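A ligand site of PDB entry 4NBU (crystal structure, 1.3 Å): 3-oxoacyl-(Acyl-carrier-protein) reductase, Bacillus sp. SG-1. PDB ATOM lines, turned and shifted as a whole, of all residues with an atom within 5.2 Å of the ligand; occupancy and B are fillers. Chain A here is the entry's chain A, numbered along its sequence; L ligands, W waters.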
ATOM      1  N   GLY A  20     -16.966   0.714 -16.497  1.00  0.00           N
ATOM      2  CA  GLY A  20     -15.829  -0.043 -16.009  1.00  0.00           C
ATOM      3  C   GLY A  20     -16.154  -1.171 -15.048  1.00  0.00           C
ATOM      4  O   GLY A  20     -15.283  -1.606 -14.301  1.00  0.00           O
ATOM      5  N   ALA A  21     -17.392  -1.678 -15.073  1.00  0.00           N
ATOM      6  CA  ALA A  21     -17.809  -2.639 -14.074  1.00  0.00           C
ATOM      7  C   ALA A  21     -17.594  -4.109 -14.446  1.00  0.00           C
ATOM      8  O   ALA A  21     -18.155  -4.987 -13.801  1.00  0.00           O
ATOM      9  CB  ALA A  21     -19.271  -2.392 -13.662  1.00  0.00           C
ATOM     10  N   ALA A  22     -16.774  -4.377 -15.462  1.00  0.00           N
ATOM     11  CA  ALA A  22     -16.466  -5.767 -15.787  1.00  0.00           C
ATOM     12  C   ALA A  22     -15.373  -6.341 -14.891  1.00  0.00           C
ATOM     13  O   ALA A  22     -15.171  -7.553 -14.836  1.00  0.00           O
ATOM     14  CB  ALA A  22     -16.111  -5.922 -17.246  1.00  0.00           C
ATOM     15  N   ASN A  23     -14.680  -5.468 -14.163  1.00  0.00           N
ATOM     16  CA  ASN A  23     -13.569  -5.872 -13.303  1.00  0.00           C
ATOM     17  C   ASN A  23     -13.507  -4.995 -12.069  1.00  0.00           C
ATOM     18  O   ASN A  23     -14.101  -3.922 -12.036  1.00  0.00           O
ATOM     19  CB  ASN A  23     -12.241  -5.699 -14.038  1.00  0.00           C
ATOM     20  CG  ASN A  23     -12.072  -6.658 -15.193  1.00  0.00           C
ATOM     21  OD1 ASN A  23     -11.786  -7.842 -14.992  1.00  0.00           O
ATOM     22  ND2 ASN A  23     -12.238  -6.153 -16.408  1.00  0.00           N
ATOM     23  N   GLY A  24     -12.769  -5.458 -11.062  1.00  0.00           N
ATOM     24  CA  GLY A  24     -12.320  -4.601  -9.963  1.00  0.00           C
ATOM     25  C   GLY A  24     -13.402  -3.946  -9.132  1.00  0.00           C
ATOM     26  O   GLY A  24     -14.395  -4.581  -8.758  1.00  0.00           O
ATOM     27  N   ILE A  25     -13.193  -2.667  -8.840  1.00  0.00           N
ATOM     28  CA  ILE A  25     -14.138  -1.916  -8.025  1.00  0.00           C
ATOM     29  C   ILE A  25     -15.542  -1.923  -8.628  1.00  0.00           C
ATOM     30  O   ILE A  25     -16.526  -2.159  -7.939  1.00  0.00           O
ATOM     31  CB  ILE A  25     -13.631  -0.470  -7.844  1.00  0.00           C
ATOM     32  CG1 ILE A  25     -12.375  -0.473  -6.965  1.00  0.00           C
ATOM     33  CG2 ILE A  25     -14.731   0.390  -7.245  1.00  0.00           C
ATOM     34  CD1 ILE A  25     -11.546   0.790  -7.096  1.00  0.00           C
ATOM     35  N   GLY A  26     -15.614  -1.666  -9.938  1.00  0.00           N
ATOM     36  CA  GLY A  26     -16.898  -1.570 -10.619  1.00  0.00           C
ATOM     37  C   GLY A  26     -17.690  -2.865 -10.575  1.00  0.00           C
ATOM     38  O   GLY A  26     -18.905  -2.843 -10.375  1.00  0.00           O
ATOM     39  N   ALA A  43     -21.130  -1.379 -18.057  1.00  0.00           N
ATOM     40  CA  ALA A  43     -20.736  -0.793 -19.324  1.00  0.00           C
ATOM     41  C   ALA A  43     -19.219  -0.780 -19.382  1.00  0.00           C
ATOM     42  O   ALA A  43     -18.590  -0.060 -18.619  1.00  0.00           O
ATOM     43  CB  ALA A  43     -21.298   0.611 -19.431  1.00  0.00           C
ATOM     44  N   ASP A  44     -18.633  -1.575 -20.275  1.00  0.00           N
ATOM     45  CA  ASP A  44     -17.192  -1.799 -20.256  1.00  0.00           C
ATOM     46  C   ASP A  44     -16.782  -2.216 -21.667  1.00  0.00           C
ATOM     47  O   ASP A  44     -17.611  -2.705 -22.440  1.00  0.00           O
ATOM     48  CB  ASP A  44     -16.880  -2.900 -19.238  1.00  0.00           C
ATOM     49  CG  ASP A  44     -15.433  -2.885 -18.749  1.00  0.00           C
ATOM     50  OD1 ASP A  44     -14.511  -3.102 -19.562  1.00  0.00           O
ATOM     51  OD2 ASP A  44     -15.241  -2.711 -17.524  1.00  0.00           O
ATOM     52  N   PHE A  45     -15.511  -2.021 -22.041  1.00  0.00           N
ATOM     53  CA  PHE A  45     -15.065  -2.497 -23.353  1.00  0.00           C
ATOM     54  C   PHE A  45     -14.648  -3.963 -23.345  1.00  0.00           C
ATOM     55  O   PHE A  45     -14.556  -4.593 -24.395  1.00  0.00           O
ATOM     56  CB  PHE A  45     -13.914  -1.637 -23.924  1.00  0.00           C
ATOM     57  CG  PHE A  45     -12.569  -1.901 -23.291  1.00  0.00           C
ATOM     58  CD1 PHE A  45     -11.763  -2.958 -23.704  1.00  0.00           C
ATOM     59  CD2 PHE A  45     -12.081  -1.058 -22.312  1.00  0.00           C
ATOM     60  CE1 PHE A  45     -10.526  -3.191 -23.124  1.00  0.00           C
ATOM     61  CE2 PHE A  45     -10.844  -1.291 -21.732  1.00  0.00           C
ATOM     62  CZ  PHE A  45     -10.069  -2.347 -22.135  1.00  0.00           C
ATOM     63  N   ASN A  46     -14.346  -4.470 -22.162  1.00  0.00           N
ATOM     64  CA  ASN A  46     -13.784  -5.807 -22.034  1.00  0.00           C
ATOM     65  C   ASN A  46     -14.898  -6.846 -22.124  1.00  0.00           C
ATOM     66  O   ASN A  46     -15.569  -7.149 -21.138  1.00  0.00           O
ATOM     67  CB  ASN A  46     -13.036  -5.901 -20.688  1.00  0.00           C
ATOM     68  CG  ASN A  46     -12.324  -7.232 -20.493  1.00  0.00           C
ATOM     69  OD1 ASN A  46     -12.687  -8.252 -21.073  1.00  0.00           O
ATOM     70  ND2 ASN A  46     -11.314  -7.221 -19.622  1.00  0.00           N
ATOM     71  N   VAL A  65     -19.183  -0.775 -24.196  1.00  0.00           N
ATOM     72  CA  VAL A  65     -18.981   0.650 -24.431  1.00  0.00           C
ATOM     73  C   VAL A  65     -17.500   0.968 -24.351  1.00  0.00           C
ATOM     74  O   VAL A  65     -16.751   0.321 -23.611  1.00  0.00           O
ATOM     75  CB  VAL A  65     -19.738   1.517 -23.384  1.00  0.00           C
ATOM     76  CG1 VAL A  65     -19.015   1.533 -22.033  1.00  0.00           C
ATOM     77  CG2 VAL A  65     -19.891   2.946 -23.886  1.00  0.00           C
ATOM     78  N   ASP A  66     -17.083   1.937 -25.149  1.00  0.00           N
ATOM     79  CA  ASP A  66     -15.814   2.618 -24.938  1.00  0.00           C
ATOM     80  C   ASP A  66     -16.187   4.031 -24.524  1.00  0.00           C
ATOM     81  O   ASP A  66     -16.724   4.789 -25.345  1.00  0.00           O
ATOM     82  CB  ASP A  66     -14.999   2.637 -26.238  1.00  0.00           C
ATOM     83  CG  ASP A  66     -13.622   3.233 -26.057  1.00  0.00           C
ATOM     84  OD1 ASP A  66     -13.394   3.998 -25.092  1.00  0.00           O
ATOM     85  OD2 ASP A  66     -12.739   2.968 -26.902  1.00  0.00           O
ATOM     86  N   VAL A  67     -15.940   4.398 -23.268  1.00  0.00           N
ATOM     87  CA  VAL A  67     -16.369   5.709 -22.768  1.00  0.00           C
ATOM     88  C   VAL A  67     -15.693   6.873 -23.468  1.00  0.00           C
ATOM     89  O   VAL A  67     -16.184   7.996 -23.404  1.00  0.00           O
ATOM     90  CB  VAL A  67     -16.221   5.848 -21.244  1.00  0.00           C
ATOM     91  CG1 VAL A  67     -17.057   4.795 -20.518  1.00  0.00           C
ATOM     92  CG2 VAL A  67     -14.751   5.776 -20.824  1.00  0.00           C
ATOM     93  N   SER A  68     -14.570   6.616 -24.136  1.00  0.00           N
ATOM     94  CA  SER A  68     -13.870   7.668 -24.860  1.00  0.00           C
ATOM     95  C   SER A  68     -14.477   7.908 -26.240  1.00  0.00           C
ATOM     96  O   SER A  68     -14.122   8.861 -26.934  1.00  0.00           O
ATOM     97  CB  SER A  68     -12.372   7.339 -24.958  1.00  0.00           C
ATOM     98  OG  SER A  68     -12.124   6.279 -25.887  1.00  0.00           O
ATOM     99  N   ASN A  93     -16.899   5.140 -13.403  1.00  0.00           N
ATOM    100  CA  ASN A  93     -15.852   4.370 -12.730  1.00  0.00           C
ATOM    101  C   ASN A  93     -14.765   3.867 -13.695  1.00  0.00           C
ATOM    102  O   ASN A  93     -13.663   3.539 -13.251  1.00  0.00           O
ATOM    103  CB  ASN A  93     -16.533   3.241 -11.924  1.00  0.00           C
ATOM    104  CG  ASN A  93     -15.581   2.128 -11.492  1.00  0.00           C
ATOM    105  OD1 ASN A  93     -15.039   2.135 -10.390  1.00  0.00           O
ATOM    106  ND2 ASN A  93     -15.411   1.126 -12.358  1.00  0.00           N
ATOM    107  N   ALA A  94     -15.067   3.795 -14.994  1.00  0.00           N
ATOM    108  CA  ALA A  94     -14.048   3.376 -15.960  1.00  0.00           C
ATOM    109  C   ALA A  94     -12.793   4.238 -15.867  1.00  0.00           C
ATOM    110  O   ALA A  94     -12.882   5.456 -15.763  1.00  0.00           O
ATOM    111  CB  ALA A  94     -14.611   3.402 -17.380  1.00  0.00           C
ATOM    112  N   GLY A  95     -11.635   3.606 -15.893  1.00  0.00           N
ATOM    113  CA  GLY A  95     -10.395   4.363 -15.905  1.00  0.00           C
ATOM    114  C   GLY A  95      -9.220   3.503 -16.303  1.00  0.00           C
ATOM    115  O   GLY A  95      -9.274   2.280 -16.192  1.00  0.00           O
ATOM    116  N   ILE A  96      -8.168   4.165 -16.773  1.00  0.00           N
ATOM    117  CA  ILE A  96      -6.895   3.535 -17.126  1.00  0.00           C
ATOM    118  C   ILE A  96      -5.712   4.323 -16.565  1.00  0.00           C
ATOM    119  O   ILE A  96      -5.844   5.500 -16.201  1.00  0.00           O
ATOM    120  CB  ILE A  96      -6.686   3.396 -18.656  1.00  0.00           C
ATOM    121  CG1 ILE A  96      -6.801   4.769 -19.343  1.00  0.00           C
ATOM    122  CG2 ILE A  96      -7.650   2.379 -19.237  1.00  0.00           C
ATOM    123  CD1 ILE A  96      -6.276   4.810 -20.783  1.00  0.00           C
ATOM    124  N   VAL A 116     -10.035   8.917 -21.673  1.00  0.00           N
ATOM    125  CA  VAL A 116     -10.833   7.940 -20.948  1.00  0.00           C
ATOM    126  C   VAL A 116     -11.269   8.489 -19.596  1.00  0.00           C
ATOM    127  O   VAL A 116     -12.440   8.442 -19.236  1.00  0.00           O
ATOM    128  CB  VAL A 116     -10.060   6.623 -20.715  1.00  0.00           C
ATOM    129  CG1 VAL A 116     -10.843   5.663 -19.832  1.00  0.00           C
ATOM    130  CG2 VAL A 116      -9.733   5.958 -22.038  1.00  0.00           C
ATOM    131  N   ASN A 117     -10.313   9.009 -18.830  1.00  0.00           N
ATOM    132  CA  ASN A 117     -10.554   9.319 -17.436  1.00  0.00           C
ATOM    133  C   ASN A 117     -11.196  10.682 -17.203  1.00  0.00           C
ATOM    134  O   ASN A 117     -11.714  10.942 -16.121  1.00  0.00           O
ATOM    135  CB  ASN A 117      -9.248   9.251 -16.609  1.00  0.00           C
ATOM    136  CG  ASN A 117      -8.643   7.866 -16.545  1.00  0.00           C
ATOM    137  OD1 ASN A 117      -9.030   6.952 -17.293  1.00  0.00           O
ATOM    138  ND2 ASN A 117      -7.679   7.694 -15.657  1.00  0.00           N
ATOM    139  N   THR A 143     -15.557   8.764 -10.162  1.00  0.00           N
ATOM    140  CA  THR A 143     -14.413   8.186  -9.479  1.00  0.00           C
ATOM    141  C   THR A 143     -13.170   9.015  -9.744  1.00  0.00           C
ATOM    142  O   THR A 143     -12.659   9.064 -10.872  1.00  0.00           O
ATOM    143  CB  THR A 143     -14.180   6.742  -9.936  1.00  0.00           C
ATOM    144  OG1 THR A 143     -15.416   6.017  -9.858  1.00  0.00           O
ATOM    145  CG2 THR A 143     -13.144   6.085  -9.037  1.00  0.00           C
ATOM    146  N   SER A 144     -12.686   9.683  -8.708  1.00  0.00           N
ATOM    147  CA  SER A 144     -11.409  10.382  -8.763  1.00  0.00           C
ATOM    148  C   SER A 144     -10.330   9.459  -8.189  1.00  0.00           C
ATOM    149  O   SER A 144     -10.367   8.242  -8.443  1.00  0.00           O
ATOM    150  CB  SER A 144     -11.534  11.713  -8.008  1.00  0.00           C
ATOM    151  OG  SER A 144     -10.336  12.459  -8.078  1.00  0.00           O
ATOM    152  N   SER A 145      -9.393  10.006  -7.417  1.00  0.00           N
ATOM    153  CA  SER A 145      -8.306   9.226  -6.824  1.00  0.00           C
ATOM    154  C   SER A 145      -7.524  10.099  -5.865  1.00  0.00           C
ATOM    155  O   SER A 145      -7.440  11.309  -6.066  1.00  0.00           O
ATOM    156  CB  SER A 145      -7.328   8.745  -7.912  1.00  0.00           C
ATOM    157  OG  SER A 145      -6.192   8.110  -7.311  1.00  0.00           O
ATOM    158  N   VAL A 146      -6.916   9.487  -4.854  1.00  0.00           N
ATOM    159  CA  VAL A 146      -5.935  10.201  -4.046  1.00  0.00           C
ATOM    160  C   VAL A 146      -4.808  10.810  -4.914  1.00  0.00           C
ATOM    161  O   VAL A 146      -4.201  11.819  -4.528  1.00  0.00           O
ATOM    162  CB  VAL A 146      -5.334   9.338  -2.917  1.00  0.00           C
ATOM    163  CG1 VAL A 146      -6.386   9.027  -1.853  1.00  0.00           C
ATOM    164  CG2 VAL A 146      -4.719   8.059  -3.476  1.00  0.00           C
ATOM    165  N   TYR A 158      -2.664  10.921 -15.179  1.00  0.00           N
ATOM    166  CA  TYR A 158      -3.728  10.370 -14.351  1.00  0.00           C
ATOM    167  C   TYR A 158      -4.136  11.398 -13.283  1.00  0.00           C
ATOM    168  O   TYR A 158      -5.322  11.577 -13.017  1.00  0.00           O
ATOM    169  CB  TYR A 158      -3.205   9.094 -13.705  1.00  0.00           C
ATOM    170  CG  TYR A 158      -4.192   8.301 -12.894  1.00  0.00           C
ATOM    171  CD1 TYR A 158      -5.026   7.368 -13.489  1.00  0.00           C
ATOM    172  CD2 TYR A 158      -4.243   8.438 -11.518  1.00  0.00           C
ATOM    173  CE1 TYR A 158      -5.916   6.619 -12.736  1.00  0.00           C
ATOM    174  CE2 TYR A 158      -5.117   7.707 -10.758  1.00  0.00           C
ATOM    175  CZ  TYR A 158      -5.947   6.792 -11.376  1.00  0.00           C
ATOM    176  OH  TYR A 158      -6.815   6.040 -10.623  1.00  0.00           O
ATOM    177  N   LYS A 162      -7.836  12.874 -12.944  1.00  0.00           N
ATOM    178  CA  LYS A 162      -8.601  12.613 -11.740  1.00  0.00           C
ATOM    179  C   LYS A 162      -8.878  13.898 -10.955  1.00  0.00           C
ATOM    180  O   LYS A 162      -9.933  14.034 -10.330  1.00  0.00           O
ATOM    181  CB  LYS A 162      -7.902  11.554 -10.877  1.00  0.00           C
ATOM    182  CG  LYS A 162      -7.858  10.166 -11.541  1.00  0.00           C
ATOM    183  CD  LYS A 162      -9.238   9.642 -11.885  1.00  0.00           C
ATOM    184  CE  LYS A 162      -9.253   8.123 -11.993  1.00  0.00           C
ATOM    185  NZ  LYS A 162     -10.607   7.625 -12.291  1.00  0.00           N
ATOM    186  N   PRO A 188     -10.797   7.016  -4.058  1.00  0.00           N
ATOM    187  CA  PRO A 188     -10.223   5.838  -3.438  1.00  0.00           C
ATOM    188  C   PRO A 188      -8.730   6.025  -3.188  1.00  0.00           C
ATOM    189  O   PRO A 188      -8.025   6.687  -3.975  1.00  0.00           O
ATOM    190  CB  PRO A 188     -10.423   4.738  -4.505  1.00  0.00           C
ATOM    191  CG  PRO A 188     -11.470   5.291  -5.439  1.00  0.00           C
ATOM    192  CD  PRO A 188     -11.194   6.760  -5.459  1.00  0.00           C
ATOM    193  N   GLY A 189      -8.270   5.430  -2.096  1.00  0.00           N
ATOM    194  CA  GLY A 189      -6.849   5.234  -1.909  1.00  0.00           C
ATOM    195  C   GLY A 189      -6.413   4.011  -2.696  1.00  0.00           C
ATOM    196  O   GLY A 189      -7.202   3.459  -3.480  1.00  0.00           O
ATOM    197  N   PHE A 190      -5.177   3.576  -2.490  1.00  0.00           N
ATOM    198  CA  PHE A 190      -4.690   2.403  -3.194  1.00  0.00           C
ATOM    199  C   PHE A 190      -5.514   1.178  -2.806  1.00  0.00           C
ATOM    200  O   PHE A 190      -5.716   0.899  -1.619  1.00  0.00           O
ATOM    201  CB  PHE A 190      -3.201   2.205  -2.957  1.00  0.00           C
ATOM    202  CG  PHE A 190      -2.367   3.345  -3.444  1.00  0.00           C
ATOM    203  CD1 PHE A 190      -2.205   3.587  -4.797  1.00  0.00           C
ATOM    204  CD2 PHE A 190      -1.747   4.188  -2.538  1.00  0.00           C
ATOM    205  CE1 PHE A 190      -1.437   4.647  -5.250  1.00  0.00           C
ATOM    206  CE2 PHE A 190      -0.973   5.261  -2.983  1.00  0.00           C
ATOM    207  CZ  PHE A 190      -0.815   5.482  -4.333  1.00  0.00           C
ATOM    208  N   THR A 191      -6.014   0.496  -3.829  1.00  0.00           N
ATOM    209  CA  THR A 191      -7.023  -0.555  -3.656  1.00  0.00           C
ATOM    210  C   THR A 191      -6.611  -1.778  -4.463  1.00  0.00           C
ATOM    211  O   THR A 191      -6.140  -1.667  -5.589  1.00  0.00           O
ATOM    212  CB  THR A 191      -8.390  -0.066  -4.150  1.00  0.00           C
ATOM    213  OG1 THR A 191      -8.779   1.073  -3.383  1.00  0.00           O
ATOM    214  CG2 THR A 191      -9.466  -1.142  -3.993  1.00  0.00           C
ATOM    215  N   GLU A 192      -6.805  -2.958  -3.870  1.00  0.00           N
ATOM    216  CA  GLU A 192      -6.418  -4.227  -4.497  1.00  0.00           C
ATOM    217  C   GLU A 192      -7.247  -4.580  -5.735  1.00  0.00           C
ATOM    218  O   GLU A 192      -8.258  -5.281  -5.634  1.00  0.00           O
ATOM    219  CB  GLU A 192      -6.517  -5.357  -3.478  1.00  0.00           C
ATOM    220  CG  GLU A 192      -5.661  -5.153  -2.239  1.00  0.00           C
ATOM    221  CD  GLU A 192      -5.777  -6.306  -1.267  1.00  0.00           C
ATOM    222  OE1 GLU A 192      -6.520  -7.262  -1.558  1.00  0.00           O
ATOM    223  OE2 GLU A 192      -5.102  -6.263  -0.213  1.00  0.00           O
ATOM    224  N   THR A 193      -6.796  -4.121  -6.902  1.00  0.00           N
ATOM    225  CA  THR A 193      -7.395  -4.479  -8.184  1.00  0.00           C
ATOM    226  C   THR A 193      -6.271  -4.677  -9.185  1.00  0.00           C
ATOM    227  O   THR A 193      -5.094  -4.571  -8.846  1.00  0.00           O
ATOM    228  CB  THR A 193      -8.295  -3.357  -8.740  1.00  0.00           C
ATOM    229  OG1 THR A 193      -7.473  -2.266  -9.168  1.00  0.00           O
ATOM    230  CG2 THR A 193      -9.289  -2.866  -7.694  1.00  0.00           C
ATOM    231  N   ALA A 194      -6.638  -4.966 -10.440  1.00  0.00           N
ATOM    232  CA  ALA A 194      -5.643  -5.130 -11.494  1.00  0.00           C
ATOM    233  C   ALA A 194      -4.822  -3.858 -11.697  1.00  0.00           C
ATOM    234  O   ALA A 194      -3.682  -3.932 -12.170  1.00  0.00           O
ATOM    235  CB  ALA A 194      -6.319  -5.548 -12.796  1.00  0.00           C
ATOM    236  N   MET A 195      -5.375  -2.713 -11.331  1.00  0.00           N
ATOM    237  CA  MET A 195      -4.665  -1.454 -11.520  1.00  0.00           C
ATOM    238  C   MET A 195      -3.392  -1.380 -10.663  1.00  0.00           C
ATOM    239  O   MET A 195      -2.433  -0.700 -11.012  1.00  0.00           O
ATOM    240  CB  MET A 195      -5.589  -0.255 -11.257  1.00  0.00           C
ATOM    241  CG  MET A 195      -5.074   1.040 -11.863  1.00  0.00           C
ATOM    242  SD  MET A 195      -6.317   2.336 -11.821  1.00  0.00           S
ATOM    243  CE  MET A 195      -7.220   2.025 -13.337  1.00  0.00           C
ATOM    244  N   VAL A 196      -3.397  -2.128  -9.561  1.00  0.00           N
ATOM    245  CA  VAL A 196      -2.251  -2.173  -8.653  1.00  0.00           C
ATOM    246  C   VAL A 196      -1.488  -3.504  -8.792  1.00  0.00           C
ATOM    247  O   VAL A 196      -0.399  -3.673  -8.250  1.00  0.00           O
ATOM    248  CB  VAL A 196      -2.729  -1.930  -7.185  1.00  0.00           C
ATOM    249  CG1 VAL A 196      -1.562  -1.864  -6.213  1.00  0.00           C
ATOM    250  CG2 VAL A 196      -3.510  -0.624  -7.102  1.00  0.00           C
ATOM    251  N   TYR A 226     -19.729   3.960  -3.090  1.00  0.00           N
ATOM    252  CA  TYR A 226     -20.640   4.179  -4.219  1.00  0.00           C
ATOM    253  C   TYR A 226     -22.093   3.977  -3.770  1.00  0.00           C
ATOM    254  O   TYR A 226     -22.964   4.752  -4.143  1.00  0.00           O
ATOM    255  CB  TYR A 226     -20.359   3.204  -5.363  1.00  0.00           C
ATOM    256  CG  TYR A 226     -19.070   3.389  -6.151  1.00  0.00           C
ATOM    257  CD1 TYR A 226     -18.225   4.471  -5.951  1.00  0.00           C
ATOM    258  CD2 TYR A 226     -18.708   2.458  -7.111  1.00  0.00           C
ATOM    259  CE1 TYR A 226     -17.062   4.599  -6.698  1.00  0.00           C
ATOM    260  CE2 TYR A 226     -17.554   2.584  -7.846  1.00  0.00           C
ATOM    261  CZ  TYR A 226     -16.734   3.651  -7.614  1.00  0.00           C
ATOM    262  OH  TYR A 226     -15.587   3.798  -8.343  1.00  0.00           O
HETATM  263  P1  LIG L   1      -9.731  -2.239 -13.077  1.00  0.00           P
HETATM  264  O1  LIG L   1      -8.650  -2.278 -14.131  1.00  0.00           O
HETATM  265  O2  LIG L   1      -9.874  -3.519 -12.339  1.00  0.00           O
HETATM  266  O3  LIG L   1     -11.101  -1.837 -13.730  1.00  0.00           O
HETATM  267  C1  LIG L   1     -11.151  -0.821 -14.679  1.00  0.00           C
HETATM  268  C2  LIG L   1     -12.260  -1.168 -15.670  1.00  0.00           C
HETATM  269  O4  LIG L   1     -12.513  -0.083 -16.494  1.00  0.00           O
HETATM  270  C3  LIG L   1     -11.901  -2.358 -16.501  1.00  0.00           C
HETATM  271  O5  LIG L   1     -12.887  -3.348 -16.469  1.00  0.00           O
HETATM  272  C4  LIG L   1     -11.699  -1.751 -17.848  1.00  0.00           C
HETATM  273  O6  LIG L   1     -11.986  -2.584 -18.933  1.00  0.00           O
HETATM  274  C5  LIG L   1     -12.598  -0.573 -17.795  1.00  0.00           C
HETATM  275  N1  LIG L   1     -12.257   0.427 -18.799  1.00  0.00           N
HETATM  276  C6  LIG L   1     -11.062   1.025 -18.998  1.00  0.00           C
HETATM  277  N2  LIG L   1     -11.156   1.867 -20.032  1.00  0.00           N
HETATM  278  C7  LIG L   1     -12.407   1.831 -20.521  1.00  0.00           C
HETATM  279  C8  LIG L   1     -13.097   2.467 -21.544  1.00  0.00           C
HETATM  280  N3  LIG L   1     -12.438   3.388 -22.420  1.00  0.00           N
HETATM  281  N4  LIG L   1     -14.396   2.210 -21.767  1.00  0.00           N
HETATM  282  C9  LIG L   1     -15.069   1.343 -21.000  1.00  0.00           C
HETATM  283  N5  LIG L   1     -14.445   0.684 -19.983  1.00  0.00           N
HETATM  284  C10 LIG L   1     -13.136   0.918 -19.726  1.00  0.00           C
HETATM  285  O7  LIG L   1      -9.309  -1.111 -12.028  1.00  0.00           O
HETATM  286  P2  LIG L   1     -10.085  -0.478 -10.794  1.00  0.00           P
HETATM  287  O8  LIG L   1      -9.042  -0.367  -9.737  1.00  0.00           O
HETATM  288  O9  LIG L   1     -11.269  -1.303 -10.419  1.00  0.00           O
HETATM  289  O10 LIG L   1     -10.539   0.929 -11.349  1.00  0.00           O
HETATM  290  C11 LIG L   1     -11.816   1.434 -11.190  1.00  0.00           C
HETATM  291  C12 LIG L   1     -11.650   2.997 -10.970  1.00  0.00           C
HETATM  292  O11 LIG L   1     -11.057   3.312  -9.682  1.00  0.00           O
HETATM  293  C13 LIG L   1     -10.822   3.742 -12.055  1.00  0.00           C
HETATM  294  O12 LIG L   1     -11.430   4.912 -12.430  1.00  0.00           O
HETATM  295  C14 LIG L   1      -9.556   3.942 -11.338  1.00  0.00           C
HETATM  296  O13 LIG L   1      -8.828   4.972 -11.907  1.00  0.00           O
HETATM  297  C15 LIG L   1     -10.044   4.235  -9.947  1.00  0.00           C
HETATM  298  N6  LIG L   1      -9.076   4.217  -8.879  1.00  0.00           N
HETATM  299  C16 LIG L   1      -8.396   3.003  -8.609  1.00  0.00           C
HETATM  300  C17 LIG L   1      -7.565   2.888  -7.535  1.00  0.00           C
HETATM  301  C18 LIG L   1      -6.847   1.627  -7.228  1.00  0.00           C
HETATM  302  O14 LIG L   1      -5.880   1.649  -6.479  1.00  0.00           O
HETATM  303  N7  LIG L   1      -7.259   0.373  -7.773  1.00  0.00           N
HETATM  304  C19 LIG L   1      -7.322   4.025  -6.605  1.00  0.00           C
HETATM  305  C20 LIG L   1      -8.034   5.288  -6.983  1.00  0.00           C
HETATM  306  C21 LIG L   1      -8.847   5.343  -8.069  1.00  0.00           C
HETATM  307  O   HOH W   1      -9.409   2.447 -22.372  1.00  0.00           O
HETATM  308  O   HOH W   2      -7.790   0.024 -16.287  1.00  0.00           O
HETATM  309  O   HOH W   3     -13.583  -1.077 -11.910  1.00  0.00           O
HETATM  310  O   HOH W   4      -6.161  -1.983 -14.682  1.00  0.00           O
HETATM  311  O   HOH W   5      -8.908  -4.619 -15.872  1.00  0.00           O
HETATM  312  O   HOH W   6      -5.382   5.734  -8.337  1.00  0.00           O
HETATM  313  O   HOH W   7      -9.312  -5.664 -11.171  1.00  0.00           O
HETATM  314  O   HOH W   8     -10.245  -4.691 -18.872  1.00  0.00           O
HETATM  315  O   HOH W   9     -13.426   6.967 -13.601  1.00  0.00           O
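Gly 20 touches the ligand (O to C2, 3.3 Å). CA of Gly 24 touches O9 of the ligand, at 3.5 Å. Phe 45 touches the ligand. CB of Asn 46 touches O6 of the ligand, 3.9 Å away. Val 65 touches the ligand (O to C9, 3.3 Å). Ala 94 touches the ligand (O to O12, 3.7 Å). Gly 95 touches the ligand. Ile 96 touches the ligand (CG2 to N2, 3.6 Å). Val 116 touches the ligand. Thr 143 touches the ligand. Ser 144 touches the ligand. OG of Ser 145 touches C20 of the ligand, 3.4 Å away. Pro 188 touches the ligand. O of Gly 189 touches C19 of the ligand (3.2 Å). Phe 190 touches the ligand (CA to O14, 3.6 Å). CG2 of Val 196 touches O14 of the ligand, 3.3 Å away. Hydrophobic or aromatic side chains that line the ligand: Ile 25, Phe 45, Val 67, Ala 94, Ile 96, Val 116, Tyr 158, Pro 188, Met 195 and Val 196. 27 residues have an atom within 4 Å of the ligand: Gly 20, Asn 23, Gly 24, Ile 25, Asp 44, Phe 45, Asn 46, Val 65, Asp 66, Val 67, Asn 93, Ala 94, Gly 95, Ile 96, Val 116, Thr 143, Ser 144, Ser 145, Tyr 158, Lys 162, Pro 188, Gly 189, Phe 190, Thr 191, Thr 193, Met 195 and Val 196. The nearest printed residue that does not touch the ligand is Ala 194 (4.02 Å).
OD2 of Asp 44 is in hydrogen-bond range of N of Ala 21 (3.4 Å). O of Gly 20 lies within hydrogen-bond range of ND2 of Asn 93 (3.4 Å). The side-chain amide oxygen (OD1) of Asn 93 lies within hydrogen-bond range of the side-chain hydroxyl (OH) of Tyr 226 (2.7 Å). O of Lys 162 is in hydrogen-bond range of OG of Ser 144, at 2.8 Å. NZ of Lys 162 lies within hydrogen-bond range of O of Thr 143 (2.9 Å). OG1 of Thr 191 sits at hydrogen-bond distance from O of Gly 189 (2.9 Å). N of Phe 45 lies within hydrogen-bond range of O of Val 65 (3.1 Å). The side-chain hydroxyl (OH) of Tyr 226 is in hydrogen-bond range of the side-chain hydroxyl (OG1) of Thr 143.
Water W7 lies within hydrogen-bond range of O2 of the ligand (2.5 Å), N of Ala 194 (2.9 Å) and N of Gly 24 (3.5 Å). Water W8 lies within hydrogen-bond range of O6 of the ligand, ND2 of Asn 46 and ND2 of Asn 23. Water W6 bridges the side-chain hydroxyl of Ser 145 (2.7 Å) and the side-chain hydroxyl of Tyr 158 (2.7 Å). Water W9 lies within hydrogen-bond range of O of Ala 94 (2.7 Å), O12 of the ligand (3.1 Å), NZ of Lys 162 (3.2 Å) and O of Asn 93 (3.5 Å). Water W2 lies within hydrogen-bond range of O of Gly 95 and O1 of the ligand.
O8 of the ligand sits at hydrogen-bond distance from OG1 of Thr 193, at 2.5 Å. An oxygen (O13) of the ligand sits at hydrogen-bond distance from the side-chain hydroxyl (OH) of Tyr 158, at 2.6 Å. The side-chain carboxylate (OD1) of Asp 44 sits at hydrogen-bond distance from an oxygen (O6) of the ligand, 2.7 Å away. The backbone carbonyl oxygen of Asn 93 sits at hydrogen-bond distance from an oxygen (O12) of the ligand, 2.7 Å away. N of Ile 25 lies within hydrogen-bond range of O9 of the ligand. NZ of Lys 162 sits at hydrogen-bond distance from O12 of the ligand (2.8 Å). The side-chain amide nitrogen (ND2) of Asn 23 is in hydrogen-bond range of an oxygen (O5) of the ligand (2.9 Å). The backbone NH (N) of Thr 191 sits at hydrogen-bond distance from an oxygen (O14) of the ligand (2.9 Å). N7 of the ligand sits at hydrogen-bond distance from O of Thr 191. The side-chain carboxylate of Asp 66 sits at hydrogen-bond distance from a nitrogen (N3) of the ligand. N4 of the ligand is in hydrogen-bond range of N of Val 67. O13 of the ligand lies within hydrogen-bond range of SD of Met 195.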
